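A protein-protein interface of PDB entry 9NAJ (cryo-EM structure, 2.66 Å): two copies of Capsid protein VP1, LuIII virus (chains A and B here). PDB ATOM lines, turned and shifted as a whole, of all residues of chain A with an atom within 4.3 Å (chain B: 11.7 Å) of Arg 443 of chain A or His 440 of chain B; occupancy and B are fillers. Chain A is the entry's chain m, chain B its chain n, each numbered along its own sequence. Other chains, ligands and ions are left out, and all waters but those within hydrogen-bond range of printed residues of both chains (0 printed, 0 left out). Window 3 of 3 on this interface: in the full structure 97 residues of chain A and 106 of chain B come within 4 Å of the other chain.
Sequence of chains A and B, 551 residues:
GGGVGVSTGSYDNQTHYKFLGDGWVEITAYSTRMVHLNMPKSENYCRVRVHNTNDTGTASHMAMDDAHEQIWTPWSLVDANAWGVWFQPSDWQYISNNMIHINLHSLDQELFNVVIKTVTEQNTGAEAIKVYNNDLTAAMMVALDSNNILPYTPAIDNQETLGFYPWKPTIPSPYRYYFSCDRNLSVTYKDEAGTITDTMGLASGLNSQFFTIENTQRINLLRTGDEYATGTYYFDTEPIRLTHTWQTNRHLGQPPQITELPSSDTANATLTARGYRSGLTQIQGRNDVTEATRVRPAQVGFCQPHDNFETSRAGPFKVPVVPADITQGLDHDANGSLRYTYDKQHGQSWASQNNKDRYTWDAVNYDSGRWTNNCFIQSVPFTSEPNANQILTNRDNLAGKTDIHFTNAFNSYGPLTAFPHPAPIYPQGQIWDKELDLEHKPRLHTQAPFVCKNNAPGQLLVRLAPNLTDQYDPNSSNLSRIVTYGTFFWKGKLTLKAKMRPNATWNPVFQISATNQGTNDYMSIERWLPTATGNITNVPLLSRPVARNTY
The backbone NH (N) of Phe 419 of chain A is in hydrogen-bond range of the backbone carbonyl oxygen (O) of His 440 of chain B (3.2 Å). A ring nitrogen (NE2) of His 440 of chain B is in hydrogen-bond range of the backbone carbonyl oxygen (O) of Arg 443 of chain A, 3.3 Å away.
Tyr 413 of chain A touches its own counterpart, Tyr 413 of chain B. Arg 443 of chain A touches Lys 441 of chain B, but with the chains exchanged Lys 441 of chain A does not touch Arg 443 of chain B (10.4 Å). Positions printed for both chains: 413, 441, 442, 443 and 444. Of the 11 pairs that touch across the chains among the printed residues, 1 has its exchanged pair printed and touching as well.
O of Leu 438 of chain B is in hydrogen-bond range of NZ of Lys 441 of chain B (3.2 Å).
Of the 8 printed residues of chain A, 6 touch a printed residue of chain B. Printed residues of chain A that touch a printed residue of chain B: Tyr 413, Ala 418, Phe 419, His 421, Arg 443 and Leu 444. Of the 17 printed residues of chain B, 6 touch a printed residue of chain A. Hydrophobic or aromatic side chains of chain B that line the printed part of chain A: Tyr 413, Leu 438, His 440 and Pro 442. Among the printed residues, 11 pairs touch across the chains.
Tyr 413 of chain A touches Tyr 413 of chain B. Ala 418 of chain A touches Leu 438 of chain B. His 440 of chain B touches Ala 418 of chain A. Ala 418 of chain A touches Pro 442 of chain B. Phe 419 of chain A touches Leu 438 of chain B. Glu 439 of chain B touches His 421 of chain A. CB of His 421 of chain A touches CE1 of His 440 of chain B, 3.6 Å away. Arg 443 of chain A touches Lys 441 of chain B (NH2 to O, 3.8 Å). NE2 of His 440 of chain B touches CB of Leu 444 of chain A, 3.4 Å away.
Arg 443 of chain A touches two residues of chain B. Of chain B, only Glu 439 (3.6 Å) and His 440 (3.6 Å) come within 4 Å of His 421 of chain A. Printed residues of chain B within 4 Å of Leu 444 of chain A: His 440 (3.4 Å). Of the printed residues of chain A, Pro 442 of chain B touches Ala 418 (3.5 Å). Of the printed residues of chain A, Tyr 413 of chain B touches Tyr 413 (3.98 Å). Lys 453 of chain B touches none of the printed residues of chain A. The nearest residue of chain B that does not touch Arg 443 of chain A is Glu 439 of chain B (5.4 Å). The nearest printed residue of chain A that does not touch Lys 441 of chain B is Ala 418 of chain A (4.4 Å).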
ATOM      1  N   TYR A 413     -24.521 -34.301 -12.266  1.00  0.00           N
ATOM      2  CA  TYR A 413     -24.518 -32.944 -11.748  1.00  0.00           C
ATOM      3  C   TYR A 413     -25.744 -32.706 -10.883  1.00  0.00           C
ATOM      4  O   TYR A 413     -26.843 -33.155 -11.205  1.00  0.00           O
ATOM      5  CB  TYR A 413     -24.480 -31.938 -12.891  1.00  0.00           C
ATOM      6  CG  TYR A 413     -24.530 -30.506 -12.446  1.00  0.00           C
ATOM      7  CD1 TYR A 413     -23.420 -29.899 -11.898  1.00  0.00           C
ATOM      8  CD2 TYR A 413     -25.674 -29.752 -12.599  1.00  0.00           C
ATOM      9  CE1 TYR A 413     -23.455 -28.596 -11.494  1.00  0.00           C
ATOM     10  CE2 TYR A 413     -25.717 -28.445 -12.203  1.00  0.00           C
ATOM     11  CZ  TYR A 413     -24.605 -27.872 -11.652  1.00  0.00           C
ATOM     12  OH  TYR A 413     -24.637 -26.563 -11.253  1.00  0.00           O
ATOM     13  N   ALA A 418     -19.365 -29.687  -6.530  1.00  0.00           N
ATOM     14  CA  ALA A 418     -18.400 -28.604  -6.425  1.00  0.00           C
ATOM     15  C   ALA A 418     -17.202 -28.953  -7.286  1.00  0.00           C
ATOM     16  O   ALA A 418     -16.734 -30.091  -7.260  1.00  0.00           O
ATOM     17  CB  ALA A 418     -17.964 -28.388  -4.978  1.00  0.00           C
ATOM     18  N   PHE A 419     -16.726 -27.995  -8.066  1.00  0.00           N
ATOM     19  CA  PHE A 419     -15.586 -28.228  -8.936  1.00  0.00           C
ATOM     20  C   PHE A 419     -14.790 -26.943  -9.048  1.00  0.00           C
ATOM     21  O   PHE A 419     -15.323 -25.855  -8.811  1.00  0.00           O
ATOM     22  CB  PHE A 419     -16.032 -28.719 -10.315  1.00  0.00           C
ATOM     23  CG  PHE A 419     -16.985 -27.805 -10.994  1.00  0.00           C
ATOM     24  CD1 PHE A 419     -16.536 -26.792 -11.802  1.00  0.00           C
ATOM     25  CD2 PHE A 419     -18.338 -27.958 -10.816  1.00  0.00           C
ATOM     26  CE1 PHE A 419     -17.415 -25.959 -12.420  1.00  0.00           C
ATOM     27  CE2 PHE A 419     -19.216 -27.124 -11.431  1.00  0.00           C
ATOM     28  CZ  PHE A 419     -18.756 -26.124 -12.233  1.00  0.00           C
ATOM     29  N   HIS A 421     -12.816 -23.910 -11.034  1.00  0.00           N
ATOM     30  CA  HIS A 421     -12.937 -23.174 -12.277  1.00  0.00           C
ATOM     31  C   HIS A 421     -11.679 -23.409 -13.102  1.00  0.00           C
ATOM     32  O   HIS A 421     -10.573 -23.324 -12.560  1.00  0.00           O
ATOM     33  CB  HIS A 421     -13.106 -21.704 -11.930  1.00  0.00           C
ATOM     34  CG  HIS A 421     -13.343 -20.807 -13.097  1.00  0.00           C
ATOM     35  ND1 HIS A 421     -13.118 -19.450 -13.036  1.00  0.00           N
ATOM     36  CD2 HIS A 421     -13.834 -21.049 -14.332  1.00  0.00           C
ATOM     37  CE1 HIS A 421     -13.424 -18.902 -14.195  1.00  0.00           C
ATOM     38  NE2 HIS A 421     -13.860 -19.852 -15.001  1.00  0.00           N
ATOM     39  N   LYS A 441     -28.159 -17.743 -16.758  1.00  0.00           N
ATOM     40  CA  LYS A 441     -26.824 -17.634 -17.289  1.00  0.00           C
ATOM     41  C   LYS A 441     -25.962 -18.785 -16.815  1.00  0.00           C
ATOM     42  O   LYS A 441     -26.196 -19.343 -15.743  1.00  0.00           O
ATOM     43  CB  LYS A 441     -26.178 -16.320 -16.842  1.00  0.00           C
ATOM     44  CG  LYS A 441     -26.817 -15.095 -17.425  1.00  0.00           C
ATOM     45  CD  LYS A 441     -26.091 -13.850 -16.992  1.00  0.00           C
ATOM     46  CE  LYS A 441     -26.633 -12.639 -17.710  1.00  0.00           C
ATOM     47  NZ  LYS A 441     -27.955 -12.242 -17.179  1.00  0.00           N
ATOM     48  N   PRO A 442     -24.957 -19.168 -17.589  1.00  0.00           N
ATOM     49  CA  PRO A 442     -24.085 -20.254 -17.159  1.00  0.00           C
ATOM     50  C   PRO A 442     -23.226 -19.809 -15.996  1.00  0.00           C
ATOM     51  O   PRO A 442     -22.928 -18.627 -15.827  1.00  0.00           O
ATOM     52  CB  PRO A 442     -23.242 -20.536 -18.400  1.00  0.00           C
ATOM     53  CG  PRO A 442     -23.205 -19.253 -19.096  1.00  0.00           C
ATOM     54  CD  PRO A 442     -24.525 -18.604 -18.874  1.00  0.00           C
ATOM     55  N   ARG A 443     -22.832 -20.778 -15.177  1.00  0.00           N
ATOM     56  CA  ARG A 443     -22.034 -20.453 -14.008  1.00  0.00           C
ATOM     57  C   ARG A 443     -20.606 -20.117 -14.401  1.00  0.00           C
ATOM     58  O   ARG A 443     -19.918 -19.372 -13.698  1.00  0.00           O
ATOM     59  CB  ARG A 443     -22.078 -21.610 -13.023  1.00  0.00           C
ATOM     60  CG  ARG A 443     -23.439 -21.795 -12.399  1.00  0.00           C
ATOM     61  CD  ARG A 443     -23.471 -23.022 -11.527  1.00  0.00           C
ATOM     62  NE  ARG A 443     -22.558 -22.914 -10.397  1.00  0.00           N
ATOM     63  CZ  ARG A 443     -22.864 -22.316  -9.256  1.00  0.00           C
ATOM     64  NH1 ARG A 443     -24.061 -21.775  -9.094  1.00  0.00           N
ATOM     65  NH2 ARG A 443     -21.975 -22.259  -8.277  1.00  0.00           N
ATOM     66  N   LEU A 444     -20.136 -20.667 -15.514  1.00  0.00           N
ATOM     67  CA  LEU A 444     -18.832 -20.313 -16.052  1.00  0.00           C
ATOM     68  C   LEU A 444     -18.855 -20.542 -17.551  1.00  0.00           C
ATOM     69  O   LEU A 444     -19.570 -21.423 -18.023  1.00  0.00           O
ATOM     70  CB  LEU A 444     -17.716 -21.131 -15.386  1.00  0.00           C
ATOM     71  CG  LEU A 444     -17.563 -22.660 -15.432  1.00  0.00           C
ATOM     72  CD1 LEU A 444     -18.852 -23.408 -15.182  1.00  0.00           C
ATOM     73  CD2 LEU A 444     -16.945 -23.128 -16.718  1.00  0.00           C
ATOM     74  N   TYR B 413     -32.575 -33.603 -11.694  1.00  0.00           N
ATOM     75  CA  TYR B 413     -32.264 -32.278 -11.185  1.00  0.00           C
ATOM     76  C   TYR B 413     -32.174 -31.281 -12.327  1.00  0.00           C
ATOM     77  O   TYR B 413     -31.638 -31.586 -13.392  1.00  0.00           O
ATOM     78  CB  TYR B 413     -30.957 -32.302 -10.404  1.00  0.00           C
ATOM     79  CG  TYR B 413     -30.531 -30.959  -9.886  1.00  0.00           C
ATOM     80  CD1 TYR B 413     -31.153 -30.394  -8.793  1.00  0.00           C
ATOM     81  CD2 TYR B 413     -29.490 -30.269 -10.469  1.00  0.00           C
ATOM     82  CE1 TYR B 413     -30.771 -29.177  -8.313  1.00  0.00           C
ATOM     83  CE2 TYR B 413     -29.096 -29.051  -9.992  1.00  0.00           C
ATOM     84  CZ  TYR B 413     -29.739 -28.510  -8.914  1.00  0.00           C
ATOM     85  OH  TYR B 413     -29.349 -27.290  -8.427  1.00  0.00           O
ATOM     86  N   GLY B 414     -32.714 -30.092 -12.108  1.00  0.00           N
ATOM     87  CA  GLY B 414     -32.767 -29.095 -13.144  1.00  0.00           C
ATOM     88  C   GLY B 414     -33.118 -27.721 -12.623  1.00  0.00           C
ATOM     89  O   GLY B 414     -33.112 -27.466 -11.418  1.00  0.00           O
ATOM     90  N   PRO B 415     -33.433 -26.803 -13.536  1.00  0.00           N
ATOM     91  CA  PRO B 415     -33.691 -25.421 -13.126  1.00  0.00           C
ATOM     92  C   PRO B 415     -34.944 -25.261 -12.297  1.00  0.00           C
ATOM     93  O   PRO B 415     -35.041 -24.302 -11.527  1.00  0.00           O
ATOM     94  CB  PRO B 415     -33.832 -24.691 -14.462  1.00  0.00           C
ATOM     95  CG  PRO B 415     -33.122 -25.522 -15.414  1.00  0.00           C
ATOM     96  CD  PRO B 415     -33.375 -26.924 -14.994  1.00  0.00           C
ATOM     97  N   LYS B 434     -16.916 -25.980   7.407  1.00  0.00           N
ATOM     98  CA  LYS B 434     -16.158 -25.038   6.606  1.00  0.00           C
ATOM     99  C   LYS B 434     -16.529 -25.218   5.145  1.00  0.00           C
ATOM    100  O   LYS B 434     -16.803 -26.332   4.698  1.00  0.00           O
ATOM    101  CB  LYS B 434     -14.656 -25.239   6.790  1.00  0.00           C
ATOM    102  CG  LYS B 434     -13.846 -24.211   6.047  1.00  0.00           C
ATOM    103  CD  LYS B 434     -12.365 -24.376   6.234  1.00  0.00           C
ATOM    104  CE  LYS B 434     -11.837 -25.466   5.354  1.00  0.00           C
ATOM    105  NZ  LYS B 434     -10.371 -25.582   5.508  1.00  0.00           N
ATOM    106  N   GLU B 435     -16.551 -24.121   4.404  1.00  0.00           N
ATOM    107  CA  GLU B 435     -16.848 -24.203   2.988  1.00  0.00           C
ATOM    108  C   GLU B 435     -15.614 -24.575   2.186  1.00  0.00           C
ATOM    109  O   GLU B 435     -14.499 -24.164   2.504  1.00  0.00           O
ATOM    110  CB  GLU B 435     -17.431 -22.889   2.479  1.00  0.00           C
ATOM    111  CG  GLU B 435     -17.725 -22.909   0.990  1.00  0.00           C
ATOM    112  CD  GLU B 435     -18.736 -23.967   0.578  1.00  0.00           C
ATOM    113  OE1 GLU B 435     -19.438 -24.525   1.436  1.00  0.00           O
ATOM    114  OE2 GLU B 435     -18.809 -24.265  -0.627  1.00  0.00           O
ATOM    115  N   LEU B 436     -15.828 -25.371   1.145  1.00  0.00           N
ATOM    116  CA  LEU B 436     -14.753 -25.764   0.253  1.00  0.00           C
ATOM    117  C   LEU B 436     -14.186 -24.541  -0.451  1.00  0.00           C
ATOM    118  O   LEU B 436     -14.890 -23.565  -0.710  1.00  0.00           O
ATOM    119  CB  LEU B 436     -15.256 -26.766  -0.774  1.00  0.00           C
ATOM    120  CG  LEU B 436     -15.356 -28.230  -0.357  1.00  0.00           C
ATOM    121  CD1 LEU B 436     -16.421 -28.427   0.687  1.00  0.00           C
ATOM    122  CD2 LEU B 436     -15.648 -29.083  -1.556  1.00  0.00           C
ATOM    123  N   ASP B 437     -12.905 -24.603  -0.779  1.00  0.00           N
ATOM    124  CA  ASP B 437     -12.199 -23.462  -1.334  1.00  0.00           C
ATOM    125  C   ASP B 437     -12.300 -23.431  -2.851  1.00  0.00           C
ATOM    126  O   ASP B 437     -11.652 -22.609  -3.498  1.00  0.00           O
ATOM    127  CB  ASP B 437     -10.740 -23.485  -0.880  1.00  0.00           C
ATOM    128  CG  ASP B 437     -10.019 -22.177  -1.133  1.00  0.00           C
ATOM    129  OD1 ASP B 437     -10.660 -21.199  -1.571  1.00  0.00           O
ATOM    130  OD2 ASP B 437      -8.800 -22.123  -0.886  1.00  0.00           O
ATOM    131  N   LEU B 438     -13.084 -24.329  -3.428  1.00  0.00           N
ATOM    132  CA  LEU B 438     -13.303 -24.353  -4.860  1.00  0.00           C
ATOM    133  C   LEU B 438     -14.062 -23.110  -5.305  1.00  0.00           C
ATOM    134  O   LEU B 438     -14.720 -22.435  -4.515  1.00  0.00           O
ATOM    135  CB  LEU B 438     -14.076 -25.608  -5.238  1.00  0.00           C
ATOM    136  CG  LEU B 438     -13.273 -26.851  -4.884  1.00  0.00           C
ATOM    137  CD1 LEU B 438     -14.071 -28.103  -5.113  1.00  0.00           C
ATOM    138  CD2 LEU B 438     -12.011 -26.863  -5.699  1.00  0.00           C
ATOM    139  N   GLU B 439     -13.945 -22.797  -6.593  1.00  0.00           N
ATOM    140  CA  GLU B 439     -14.623 -21.622  -7.126  1.00  0.00           C
ATOM    141  C   GLU B 439     -16.122 -21.834  -7.230  1.00  0.00           C
ATOM    142  O   GLU B 439     -16.908 -20.969  -6.834  1.00  0.00           O
ATOM    143  CB  GLU B 439     -14.053 -21.246  -8.486  1.00  0.00           C
ATOM    144  CG  GLU B 439     -14.781 -20.079  -9.114  1.00  0.00           C
ATOM    145  CD  GLU B 439     -14.670 -18.791  -8.320  1.00  0.00           C
ATOM    146  OE1 GLU B 439     -13.799 -18.692  -7.429  1.00  0.00           O
ATOM    147  OE2 GLU B 439     -15.481 -17.877  -8.571  1.00  0.00           O
ATOM    148  N   HIS B 440     -16.541 -22.960  -7.778  1.00  0.00           N
ATOM    149  CA  HIS B 440     -17.954 -23.262  -7.917  1.00  0.00           C
ATOM    150  C   HIS B 440     -18.350 -24.182  -6.777  1.00  0.00           C
ATOM    151  O   HIS B 440     -17.835 -25.297  -6.667  1.00  0.00           O
ATOM    152  CB  HIS B 440     -18.235 -23.871  -9.285  1.00  0.00           C
ATOM    153  CG  HIS B 440     -17.933 -22.929 -10.407  1.00  0.00           C
ATOM    154  ND1 HIS B 440     -16.663 -22.768 -10.917  1.00  0.00           N
ATOM    155  CD2 HIS B 440     -18.716 -22.046 -11.065  1.00  0.00           C
ATOM    156  CE1 HIS B 440     -16.682 -21.849 -11.863  1.00  0.00           C
ATOM    157  NE2 HIS B 440     -17.917 -21.396 -11.973  1.00  0.00           N
ATOM    158  N   LYS B 441     -19.265 -23.727  -5.958  1.00  0.00           N
ATOM    159  CA  LYS B 441     -19.474 -24.277  -4.642  1.00  0.00           C
ATOM    160  C   LYS B 441     -20.809 -24.987  -4.563  1.00  0.00           C
ATOM    161  O   LYS B 441     -21.746 -24.643  -5.285  1.00  0.00           O
ATOM    162  CB  LYS B 441     -19.445 -23.166  -3.589  1.00  0.00           C
ATOM    163  CG  LYS B 441     -18.102 -22.521  -3.419  1.00  0.00           C
ATOM    164  CD  LYS B 441     -18.135 -21.486  -2.326  1.00  0.00           C
ATOM    165  CE  LYS B 441     -16.750 -20.960  -2.046  1.00  0.00           C
ATOM    166  NZ  LYS B 441     -16.292 -20.045  -3.115  1.00  0.00           N
ATOM    167  N   PRO B 442     -20.932 -25.983  -3.699  1.00  0.00           N
ATOM    168  CA  PRO B 442     -22.207 -26.676  -3.570  1.00  0.00           C
ATOM    169  C   PRO B 442     -23.232 -25.775  -2.916  1.00  0.00           C
ATOM    170  O   PRO B 442     -22.902 -24.868  -2.152  1.00  0.00           O
ATOM    171  CB  PRO B 442     -21.866 -27.870  -2.682  1.00  0.00           C
ATOM    172  CG  PRO B 442     -20.740 -27.400  -1.880  1.00  0.00           C
ATOM    173  CD  PRO B 442     -19.935 -26.503  -2.755  1.00  0.00           C
ATOM    174  N   ARG B 443     -24.496 -26.028  -3.234  1.00  0.00           N
ATOM    175  CA  ARG B 443     -25.556 -25.196  -2.690  1.00  0.00           C
ATOM    176  C   ARG B 443     -25.795 -25.511  -1.223  1.00  0.00           C
ATOM    177  O   ARG B 443     -26.256 -24.655  -0.463  1.00  0.00           O
ATOM    178  CB  ARG B 443     -26.823 -25.385  -3.509  1.00  0.00           C
ATOM    179  CG  ARG B 443     -26.707 -24.825  -4.903  1.00  0.00           C
ATOM    180  CD  ARG B 443     -27.934 -25.141  -5.717  1.00  0.00           C
ATOM    181  NE  ARG B 443     -29.130 -24.517  -5.167  1.00  0.00           N
ATOM    182  CZ  ARG B 443     -29.500 -23.272  -5.427  1.00  0.00           C
ATOM    183  NH1 ARG B 443     -28.765 -22.521  -6.232  1.00  0.00           N
ATOM    184  NH2 ARG B 443     -30.601 -22.780  -4.884  1.00  0.00           N
ATOM    185  N   LEU B 444     -25.500 -26.738  -0.809  1.00  0.00           N
ATOM    186  CA  LEU B 444     -25.566 -27.107   0.597  1.00  0.00           C
ATOM    187  C   LEU B 444     -24.595 -28.248   0.836  1.00  0.00           C
ATOM    188  O   LEU B 444     -24.356 -29.045  -0.068  1.00  0.00           O
ATOM    189  CB  LEU B 444     -26.994 -27.503   1.001  1.00  0.00           C
ATOM    190  CG  LEU B 444     -27.804 -28.677   0.428  1.00  0.00           C
ATOM    191  CD1 LEU B 444     -27.738 -28.785  -1.078  1.00  0.00           C
ATOM    192  CD2 LEU B 444     -27.416 -29.988   1.048  1.00  0.00           C
ATOM    193  N   HIS B 445     -24.013 -28.304   2.026  1.00  0.00           N
ATOM    194  CA  HIS B 445     -23.354 -29.529   2.449  1.00  0.00           C
ATOM    195  C   HIS B 445     -24.384 -30.503   2.991  1.00  0.00           C
ATOM    196  O   HIS B 445     -25.435 -30.110   3.494  1.00  0.00           O
ATOM    197  CB  HIS B 445     -22.289 -29.252   3.497  1.00  0.00           C
ATOM    198  CG  HIS B 445     -21.184 -28.378   3.008  1.00  0.00           C
ATOM    199  ND1 HIS B 445     -20.236 -27.840   3.846  1.00  0.00           N
ATOM    200  CD2 HIS B 445     -20.898 -27.917   1.770  1.00  0.00           C
ATOM    201  CE1 HIS B 445     -19.396 -27.106   3.142  1.00  0.00           C
ATOM    202  NE2 HIS B 445     -19.779 -27.132   1.880  1.00  0.00           N
ATOM    203  N   VAL B 451     -23.057 -23.552   7.211  1.00  0.00           N
ATOM    204  CA  VAL B 451     -21.796 -23.497   6.488  1.00  0.00           C
ATOM    205  C   VAL B 451     -21.224 -22.102   6.647  1.00  0.00           C
ATOM    206  O   VAL B 451     -21.905 -21.113   6.366  1.00  0.00           O
ATOM    207  CB  VAL B 451     -21.976 -23.850   5.004  1.00  0.00           C
ATOM    208  CG1 VAL B 451     -20.680 -23.682   4.277  1.00  0.00           C
ATOM    209  CG2 VAL B 451     -22.466 -25.263   4.869  1.00  0.00           C
ATOM    210  N   LYS B 453     -19.409 -18.910   5.753  1.00  0.00           N
ATOM    211  CA  LYS B 453     -19.180 -18.308   4.445  1.00  0.00           C
ATOM    212  C   LYS B 453     -17.707 -18.007   4.221  1.00  0.00           C
ATOM    213  O   LYS B 453     -17.121 -18.432   3.220  1.00  0.00           O
ATOM    214  CB  LYS B 453     -20.012 -17.039   4.292  1.00  0.00           C
ATOM    215  CG  LYS B 453     -21.497 -17.288   4.230  1.00  0.00           C
ATOM    216  CD  LYS B 453     -22.246 -16.001   3.960  1.00  0.00           C
ATOM    217  CE  LYS B 453     -23.730 -16.254   3.772  1.00  0.00           C
ATOM    218  NZ  LYS B 453     -24.414 -16.523   5.063  1.00  0.00           N
